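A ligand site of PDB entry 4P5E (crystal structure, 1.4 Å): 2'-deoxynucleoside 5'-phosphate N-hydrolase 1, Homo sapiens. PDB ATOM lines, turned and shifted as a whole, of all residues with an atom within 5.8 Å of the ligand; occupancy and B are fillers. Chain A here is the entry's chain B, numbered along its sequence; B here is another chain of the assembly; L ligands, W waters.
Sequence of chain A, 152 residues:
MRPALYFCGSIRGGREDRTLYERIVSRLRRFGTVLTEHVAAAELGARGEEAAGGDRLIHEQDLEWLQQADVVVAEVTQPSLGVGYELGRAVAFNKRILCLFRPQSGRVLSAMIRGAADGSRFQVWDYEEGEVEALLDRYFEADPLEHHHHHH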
ATOM      1  N   TYR A   6      17.871 -22.871  19.702  1.00  0.00           N
ATOM      2  CA  TYR A   6      16.586 -22.181  19.828  1.00  0.00           C
ATOM      3  C   TYR A   6      16.848 -20.689  19.747  1.00  0.00           C
ATOM      4  O   TYR A   6      17.541 -20.128  20.614  1.00  0.00           O
ATOM      5  CB  TYR A   6      15.910 -22.547  21.138  1.00  0.00           C
ATOM      6  CG  TYR A   6      14.464 -22.131  21.282  1.00  0.00           C
ATOM      7  CD1 TYR A   6      14.125 -20.801  21.534  1.00  0.00           C
ATOM      8  CD2 TYR A   6      13.428 -23.047  21.168  1.00  0.00           C
ATOM      9  CE1 TYR A   6      12.798 -20.407  21.693  1.00  0.00           C
ATOM     10  CE2 TYR A   6      12.102 -22.675  21.330  1.00  0.00           C
ATOM     11  CZ  TYR A   6      11.794 -21.356  21.579  1.00  0.00           C
ATOM     12  OH  TYR A   6      10.470 -21.007  21.744  1.00  0.00           O
ATOM     13  N   PHE A   7      16.322 -20.039  18.710  1.00  0.00           N
ATOM     14  CA  PHE A   7      16.471 -18.605  18.539  1.00  0.00           C
ATOM     15  C   PHE A   7      15.201 -17.857  18.978  1.00  0.00           C
ATOM     16  O   PHE A   7      14.099 -18.219  18.569  1.00  0.00           O
ATOM     17  CB  PHE A   7      16.768 -18.240  17.077  1.00  0.00           C
ATOM     18  CG  PHE A   7      16.752 -16.762  16.835  1.00  0.00           C
ATOM     19  CD1 PHE A   7      17.805 -15.976  17.282  1.00  0.00           C
ATOM     20  CD2 PHE A   7      15.645 -16.163  16.264  1.00  0.00           C
ATOM     21  CE1 PHE A   7      17.759 -14.577  17.150  1.00  0.00           C
ATOM     22  CE2 PHE A   7      15.605 -14.780  16.114  1.00  0.00           C
ATOM     23  CZ  PHE A   7      16.662 -13.996  16.537  1.00  0.00           C
ATOM     24  N   CYS A   8      15.369 -16.795  19.764  1.00  0.00           N
ATOM     25  CA  CYS A   8      14.269 -15.951  20.237  1.00  0.00           C
ATOM     26  C   CYS A   8      14.389 -14.536  19.704  1.00  0.00           C
ATOM     27  O   CYS A   8      15.476 -13.970  19.721  1.00  0.00           O
ATOM     28  CB  CYS A   8      14.251 -15.825  21.772  1.00  0.00           C
ATOM     29  SG  CYS A   8      14.561 -17.346  22.722  1.00  0.00           S
ATOM     30  N   GLY A   9      13.283 -13.960  19.257  1.00  0.00           N
ATOM     31  CA  GLY A   9      13.243 -12.562  18.826  1.00  0.00           C
ATOM     32  C   GLY A   9      11.801 -12.076  18.831  1.00  0.00           C
ATOM     33  O   GLY A   9      10.882 -12.867  18.588  1.00  0.00           O
ATOM     34  N   SER A  10      11.600 -10.784  19.052  1.00  0.00           N
ATOM     35  CA  SER A  10      10.259 -10.196  19.145  1.00  0.00           C
ATOM     36  C   SER A  10       9.425 -10.433  17.896  1.00  0.00           C
ATOM     37  O   SER A  10       9.931 -10.297  16.778  1.00  0.00           O
ATOM     38  CB  SER A  10      10.393  -8.702  19.374  1.00  0.00           C
ATOM     39  OG  SER A  10       9.109  -8.080  19.452  1.00  0.00           O
ATOM     40  N   ILE A  11       8.148 -10.780  18.099  1.00  0.00           N
ATOM     41  CA  ILE A  11       7.184 -10.846  17.015  1.00  0.00           C
ATOM     42  C   ILE A  11       6.041  -9.881  17.336  1.00  0.00           C
ATOM     43  O   ILE A  11       6.003  -8.781  16.784  1.00  0.00           O
ATOM     44  CB  ILE A  11       6.688 -12.292  16.791  1.00  0.00           C
ATOM     45  CG1 ILE A  11       7.867 -13.183  16.378  1.00  0.00           C
ATOM     46  CG2 ILE A  11       5.620 -12.351  15.704  1.00  0.00           C
ATOM     47  CD1 ILE A  11       7.515 -14.656  16.270  1.00  0.00           C
ATOM     48  N   ARG A  12       5.142 -10.246  18.255  1.00  0.00           N
ATOM     49  CA  ARG A  12       4.080  -9.318  18.606  1.00  0.00           C
ATOM     50  C   ARG A  12       4.580  -8.146  19.453  1.00  0.00           C
ATOM     51  O   ARG A  12       3.903  -7.112  19.510  1.00  0.00           O
ATOM     52  CB  ARG A  12       2.918 -10.052  19.285  1.00  0.00           C
ATOM     53  CG  ARG A  12       2.093 -10.830  18.274  1.00  0.00           C
ATOM     54  CD  ARG A  12       0.831 -11.473  18.859  1.00  0.00           C
ATOM     55  NE  ARG A  12       0.115 -12.196  17.795  1.00  0.00           N
ATOM     56  CZ  ARG A  12      -0.714 -13.212  17.995  1.00  0.00           C
ATOM     57  NH1 ARG A  12      -1.286 -13.810  16.949  1.00  0.00           N
ATOM     58  NH2 ARG A  12      -0.953 -13.666  19.221  1.00  0.00           N
ATOM     59  N   GLY A  13       5.765  -8.265  20.037  1.00  0.00           N
ATOM     60  CA  GLY A  13       6.400  -7.111  20.644  1.00  0.00           C
ATOM     61  C   GLY A  13       6.833  -6.048  19.623  1.00  0.00           C
ATOM     62  O   GLY A  13       7.076  -4.893  19.983  1.00  0.00           O
ATOM     63  N   GLY A  14       6.905  -6.427  18.343  1.00  0.00           N
ATOM     64  CA  GLY A  14       7.309  -5.513  17.264  1.00  0.00           C
ATOM     65  C   GLY A  14       8.356  -6.195  16.403  1.00  0.00           C
ATOM     66  O   GLY A  14       9.210  -6.905  16.935  1.00  0.00           O
ATOM     67  N   THR A  36      13.555 -22.759  15.603  1.00  0.00           N
ATOM     68  CA  THR A  36      12.595 -21.663  15.528  1.00  0.00           C
ATOM     69  C   THR A  36      12.832 -20.788  14.314  1.00  0.00           C
ATOM     70  O   THR A  36      12.522 -19.589  14.333  1.00  0.00           O
ATOM     71  CB  THR A  36      12.671 -20.782  16.777  1.00  0.00           C
ATOM     72  OG1 THR A  36      14.024 -20.365  16.964  1.00  0.00           O
ATOM     73  CG2 THR A  36      12.210 -21.538  18.017  1.00  0.00           C
ATOM     74  N   HIS A  38      11.617 -19.572  11.868  1.00  0.00           N
ATOM     75  CA  HIS A  38      10.782 -18.504  11.342  1.00  0.00           C
ATOM     76  C   HIS A  38      10.177 -17.572  12.396  1.00  0.00           C
ATOM     77  O   HIS A  38       9.023 -17.163  12.307  1.00  0.00           O
ATOM     78  CB  HIS A  38       9.694 -19.068  10.425  1.00  0.00           C
ATOM     79  CG  HIS A  38       8.782 -20.059  11.074  1.00  0.00           C
ATOM     80  ND1 HIS A  38       7.737 -19.692  11.895  1.00  0.00           N
ATOM     81  CD2 HIS A  38       8.739 -21.406  10.985  1.00  0.00           C
ATOM     82  CE1 HIS A  38       7.098 -20.781  12.303  1.00  0.00           C
ATOM     83  NE2 HIS A  38       7.695 -21.832  11.767  1.00  0.00           N
ATOM     84  N   VAL A  39      11.000 -17.207  13.376  1.00  0.00           N
ATOM     85  CA  VAL A  39      10.843 -15.921  14.056  1.00  0.00           C
ATOM     86  C   VAL A  39      11.220 -14.860  13.017  1.00  0.00           C
ATOM     87  O   VAL A  39      10.877 -13.678  13.148  1.00  0.00           O
ATOM     88  CB  VAL A  39      11.757 -15.799  15.318  1.00  0.00           C
ATOM     89  CG1 VAL A  39      11.495 -14.471  16.075  1.00  0.00           C
ATOM     90  CG2 VAL A  39      11.577 -16.984  16.259  1.00  0.00           C
ATOM     91  N   LEU A  44       4.145 -13.486   8.692  1.00  0.00           N
ATOM     92  CA  LEU A  44       3.912 -14.282   9.890  1.00  0.00           C
ATOM     93  C   LEU A  44       2.589 -13.905  10.515  1.00  0.00           C
ATOM     94  O   LEU A  44       2.288 -12.715  10.649  1.00  0.00           O
ATOM     95  CB  LEU A  44       5.054 -14.097  10.883  1.00  0.00           C
ATOM     96  CG  LEU A  44       5.879 -15.322  11.222  1.00  0.00           C
ATOM     97  CD1 LEU A  44       6.766 -15.011  12.407  1.00  0.00           C
ATOM     98  CD2 LEU A  44       4.966 -16.496  11.551  1.00  0.00           C
ATOM     99  N   ILE A  58       0.971 -23.033  19.267  1.00  0.00           N
ATOM    100  CA  ILE A  58       2.255 -22.343  19.144  1.00  0.00           C
ATOM    101  C   ILE A  58       3.088 -22.546  20.407  1.00  0.00           C
ATOM    102  O   ILE A  58       4.254 -22.904  20.348  1.00  0.00           O
ATOM    103  CB  ILE A  58       2.046 -20.835  18.877  1.00  0.00           C
ATOM    104  CG1 ILE A  58       1.410 -20.613  17.502  1.00  0.00           C
ATOM    105  CG2 ILE A  58       3.367 -20.090  18.951  1.00  0.00           C
ATOM    106  CD1 ILE A  58       0.579 -19.346  17.433  1.00  0.00           C
ATOM    107  N   ASP A  62       6.598 -24.671  20.651  1.00  0.00           N
ATOM    108  CA  ASP A  62       7.804 -23.935  21.039  1.00  0.00           C
ATOM    109  C   ASP A  62       8.425 -24.541  22.298  1.00  0.00           C
ATOM    110  O   ASP A  62       9.643 -24.661  22.400  1.00  0.00           O
ATOM    111  CB  ASP A  62       7.515 -22.451  21.267  1.00  0.00           C
ATOM    112  CG  ASP A  62       7.443 -21.646  19.968  1.00  0.00           C
ATOM    113  OD1 ASP A  62       7.519 -22.239  18.872  1.00  0.00           O
ATOM    114  OD2 ASP A  62       7.294 -20.416  20.054  1.00  0.00           O
ATOM    115  N   PRO A  79      11.739  -4.982  23.218  1.00  0.00           N
ATOM    116  CA  PRO A  79      11.047  -5.640  24.336  1.00  0.00           C
ATOM    117  C   PRO A  79       9.873  -6.525  23.885  1.00  0.00           C
ATOM    118  O   PRO A  79       9.104  -6.147  22.989  1.00  0.00           O
ATOM    119  CB  PRO A  79      10.553  -4.468  25.175  1.00  0.00           C
ATOM    120  CG  PRO A  79      11.483  -3.322  24.864  1.00  0.00           C
ATOM    121  CD  PRO A  79      11.786  -3.513  23.383  1.00  0.00           C
ATOM    122  N   SER A  80       9.739  -7.690  24.525  1.00  0.00           N
ATOM    123  CA  SER A  80       8.816  -8.722  24.063  1.00  0.00           C
ATOM    124  C   SER A  80       8.457  -9.627  25.199  1.00  0.00           C
ATOM    125  O   SER A  80       9.367 -10.171  25.853  1.00  0.00           O
ATOM    126  CB  SER A  80       9.460  -9.555  22.935  1.00  0.00           C
ATOM    127  OG  SER A  80       8.802 -10.796  22.753  1.00  0.00           O
ATOM    128  N   LEU A  81       7.160  -9.833  25.426  1.00  0.00           N
ATOM    129  CA  LEU A  81       6.735 -10.791  26.451  1.00  0.00           C
ATOM    130  C   LEU A  81       7.168 -12.201  26.112  1.00  0.00           C
ATOM    131  O   LEU A  81       7.650 -12.941  26.963  1.00  0.00           O
ATOM    132  CB  LEU A  81       5.224 -10.757  26.604  1.00  0.00           C
ATOM    133  CG  LEU A  81       4.631  -9.456  27.154  1.00  0.00           C
ATOM    134  CD1 LEU A  81       3.157  -9.453  26.879  1.00  0.00           C
ATOM    135  CD2 LEU A  81       4.915  -9.294  28.665  1.00  0.00           C
ATOM    136  N   GLY A  82       7.010 -12.588  24.859  1.00  0.00           N
ATOM    137  CA  GLY A  82       7.340 -13.959  24.485  1.00  0.00           C
ATOM    138  C   GLY A  82       8.804 -14.283  24.589  1.00  0.00           C
ATOM    139  O   GLY A  82       9.162 -15.352  25.066  1.00  0.00           O
ATOM    140  N   VAL A  83       9.652 -13.348  24.168  1.00  0.00           N
ATOM    141  CA  VAL A  83      11.099 -13.557  24.308  1.00  0.00           C
ATOM    142  C   VAL A  83      11.463 -13.662  25.809  1.00  0.00           C
ATOM    143  O   VAL A  83      12.227 -14.542  26.203  1.00  0.00           O
ATOM    144  CB  VAL A  83      11.908 -12.427  23.640  1.00  0.00           C
ATOM    145  CG1 VAL A  83      13.383 -12.566  23.940  1.00  0.00           C
ATOM    146  CG2 VAL A  83      11.667 -12.438  22.118  1.00  0.00           C
ATOM    147  N   GLU A  86      10.330 -17.091  27.047  1.00  0.00           N
ATOM    148  CA  GLU A  86      11.245 -18.122  26.587  1.00  0.00           C
ATOM    149  C   GLU A  86      12.521 -18.144  27.424  1.00  0.00           C
ATOM    150  O   GLU A  86      12.990 -19.207  27.808  1.00  0.00           O
ATOM    151  CB  GLU A  86      11.583 -17.920  25.099  1.00  0.00           C
ATOM    152  CG  GLU A  86      10.404 -18.238  24.188  1.00  0.00           C
ATOM    153  CD  GLU A  86      10.581 -17.782  22.759  1.00  0.00           C
ATOM    154  OE1 GLU A  86      10.091 -18.509  21.853  1.00  0.00           O
ATOM    155  OE2 GLU A  86      11.190 -16.700  22.555  1.00  0.00           O
ATOM    156  N   SER B 110       0.909 -11.301  22.857  1.00  0.00           N
ATOM    157  CA  SER B 110       1.846 -12.417  22.634  1.00  0.00           C
ATOM    158  C   SER B 110       1.208 -13.798  22.637  1.00  0.00           C
ATOM    159  O   SER B 110       0.496 -14.177  23.600  1.00  0.00           O
ATOM    160  CB  SER B 110       2.898 -12.393  23.735  1.00  0.00           C
ATOM    161  OG  SER B 110       3.832 -13.470  23.550  1.00  0.00           O
ATOM    162  N   ALA B 111       1.485 -14.586  21.614  1.00  0.00           N
ATOM    163  CA  ALA B 111       0.976 -15.952  21.555  1.00  0.00           C
ATOM    164  C   ALA B 111       1.590 -16.781  22.667  1.00  0.00           C
ATOM    165  O   ALA B 111       0.983 -17.753  23.098  1.00  0.00           O
ATOM    166  CB  ALA B 111       1.270 -16.575  20.214  1.00  0.00           C
ATOM    167  N   MET B 112       2.773 -16.419  23.154  1.00  0.00           N
ATOM    168  CA  MET B 112       3.382 -17.219  24.213  1.00  0.00           C
ATOM    169  C   MET B 112       2.630 -17.046  25.510  1.00  0.00           C
ATOM    170  O   MET B 112       2.565 -17.998  26.287  1.00  0.00           O
ATOM    171  CB  MET B 112       4.866 -16.858  24.421  1.00  0.00           C
ATOM    172  CG  MET B 112       5.706 -17.183  23.208  1.00  0.00           C
ATOM    173  SD  MET B 112       5.559 -18.886  22.609  1.00  0.00           S
ATOM    174  CE  MET B 112       6.679 -19.731  23.723  1.00  0.00           C
HETATM  175  C1  LIG L   1       2.394 -17.781  15.096  1.00  0.00           C
HETATM  176  C2  LIG L   1       1.329 -17.215  14.402  1.00  0.00           C
HETATM  177  C3  LIG L   1       0.449 -18.046  13.695  1.00  0.00           C
HETATM  178  C4  LIG L   1      -0.607 -17.489  12.996  1.00  0.00           C
HETATM  179  C5  LIG L   1      -0.798 -16.105  12.985  1.00  0.00           C
HETATM  180  C6  LIG L   1       0.082 -15.275  13.692  1.00  0.00           C
HETATM  181  C7  LIG L   1       1.141 -15.835  14.401  1.00  0.00           C
HETATM  182  C8  LIG L   1       2.008 -15.002  15.101  1.00  0.00           C
HETATM  183  C9  LIG L   1       3.056 -15.571  15.809  1.00  0.00           C
HETATM  184  C10 LIG L   1       3.230 -16.969  15.830  1.00  0.00           C
HETATM  185  C11 LIG L   1       4.401 -17.558  16.574  1.00  0.00           C
HETATM  186  N1  LIG L   1       4.965 -18.718  16.139  1.00  0.00           N
HETATM  187  C12 LIG L   1       6.005 -19.269  16.734  1.00  0.00           C
HETATM  188  N2  LIG L   1       6.599 -18.737  17.815  1.00  0.00           N
HETATM  189  C13 LIG L   1       6.118 -17.576  18.294  1.00  0.00           C
HETATM  190  C14 LIG L   1       4.988 -16.943  17.720  1.00  0.00           C
HETATM  191  N3  LIG L   1       4.737 -15.829  18.450  1.00  0.00           N
HETATM  192  C15 LIG L   1       5.676 -15.790  19.433  1.00  0.00           C
HETATM  193  N4  LIG L   1       6.527 -16.841  19.368  1.00  0.00           N
HETATM  194  C16 LIG L   1       7.688 -17.123  20.117  1.00  0.00           C
HETATM  195  O1  LIG L   1       7.815 -15.940  21.167  1.00  0.00           O
HETATM  196  C17 LIG L   1       8.798 -16.907  19.317  1.00  0.00           C
HETATM  197  O2  LIG L   1       9.783 -18.012  19.328  1.00  0.00           O
HETATM  198  C18 LIG L   1       9.613 -15.600  19.679  1.00  0.00           C
HETATM  199  O3  LIG L   1      10.953 -15.745  20.014  1.00  0.00           O
HETATM  200  C19 LIG L   1       8.754 -15.005  20.821  1.00  0.00           C
HETATM  201  C20 LIG L   1       8.091 -13.729  20.314  1.00  0.00           C
HETATM  202  O4  LIG L   1       7.193 -13.269  21.361  1.00  0.00           O
HETATM  203  P1  LIG L   1       6.224 -12.026  21.111  1.00  0.00           P
HETATM  204  O5  LIG L   1       5.567 -11.832  22.458  1.00  0.00           O
HETATM  205  O6  LIG L   1       7.091 -10.848  20.720  1.00  0.00           O
HETATM  206  O7  LIG L   1       5.262 -12.366  19.991  1.00  0.00           O
HETATM  207  O   HOH W   1       3.073 -13.738  19.413  1.00  0.00           O
HETATM  208  O   HOH W   2       4.297 -20.879  14.390  1.00  0.00           O
HETATM  209  O   HOH W   3       9.296 -20.359  17.210  1.00  0.00           O
HETATM  210  O   HOH W   4       5.208  -9.229  23.435  1.00  0.00           O
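Merely in contact with the ligand: Met 112 of chain B, Cys 8, Ile 58, Ser 10, Val 39, Val 83, Tyr 6, Leu 81 and Ala 111 of chain B. Hydrophobic or aromatic side chains that line the ligand: Ile 11, Val 39, Ile 58, Val 83, Ala 111 of chain B and Met 112 of chain B.
Water W1 lies within hydrogen-bond range of an oxygen (O7) of the ligand (2.6 Å) and the backbone NH of Ala 111 of chain B (2.8 Å). Water W4 bridges O5 of the ligand and N of Leu 81. Water W3 bridges OD1 of Asp 62 and O2 of the ligand.
N of Gly 82 sits at hydrogen-bond distance from OG of Ser 80 (3.3 Å). The side-chain carboxylate of Glu 86 lies close to the side-chain sulfur of Cys 8 (3.4 Å). The side-chain hydroxyl (OG) of Ser 10 lies close to the backbone NH (N) of Gly 13 (3.4 Å). OG of Ser 110 of chain B sits close to N of Met 112 of chain B (3.2 Å). The side-chain carboxylate (OE1) of Glu 86 sits at hydrogen-bond distance from the side-chain hydroxyl (OH) of Tyr 6. The side-chain hydroxyl (OG) of Ser 10 sits at hydrogen-bond distance from the backbone carbonyl oxygen (O) of Gly 14, at 2.8 Å. The side-chain hydroxyl of Ser 80 is in hydrogen-bond range of the backbone NH of Val 83, at 3.0 Å.
The side-chain carboxylate (OE1) of Glu 86 lies within hydrogen-bond range of an oxygen (O2) of the ligand (2.6 Å). The backbone carbonyl oxygen of Gly 9 sits close to an oxygen (O3) of the ligand (3.2 Å). An oxygen (O5) of the ligand sits at hydrogen-bond distance from the side-chain hydroxyl (OG) of Ser 110 of chain B (2.6 Å). An oxygen (O6) of the ligand lies within hydrogen-bond range of the side-chain hydroxyl (OG) of Ser 80, 2.7 Å away. N2 of the ligand lies within hydrogen-bond range of OD2 of Asp 62 (2.9 Å). The backbone NH (N) of Gly 13 is in hydrogen-bond range of an oxygen (O6) of the ligand, 3.0 Å away. N of Gly 82 sits at hydrogen-bond distance from O5 of the ligand, at 2.9 Å. The backbone NH (N) of Gly 9 lies within hydrogen-bond range of an oxygen (O3) of the ligand, at 3.0 Å. The backbone NH (N) of Arg 12 lies within hydrogen-bond range of an oxygen (O7) of the ligand (2.7 Å). The backbone NH of Ile 11 lies within hydrogen-bond range of an oxygen (O6) of the ligand (2.8 Å).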
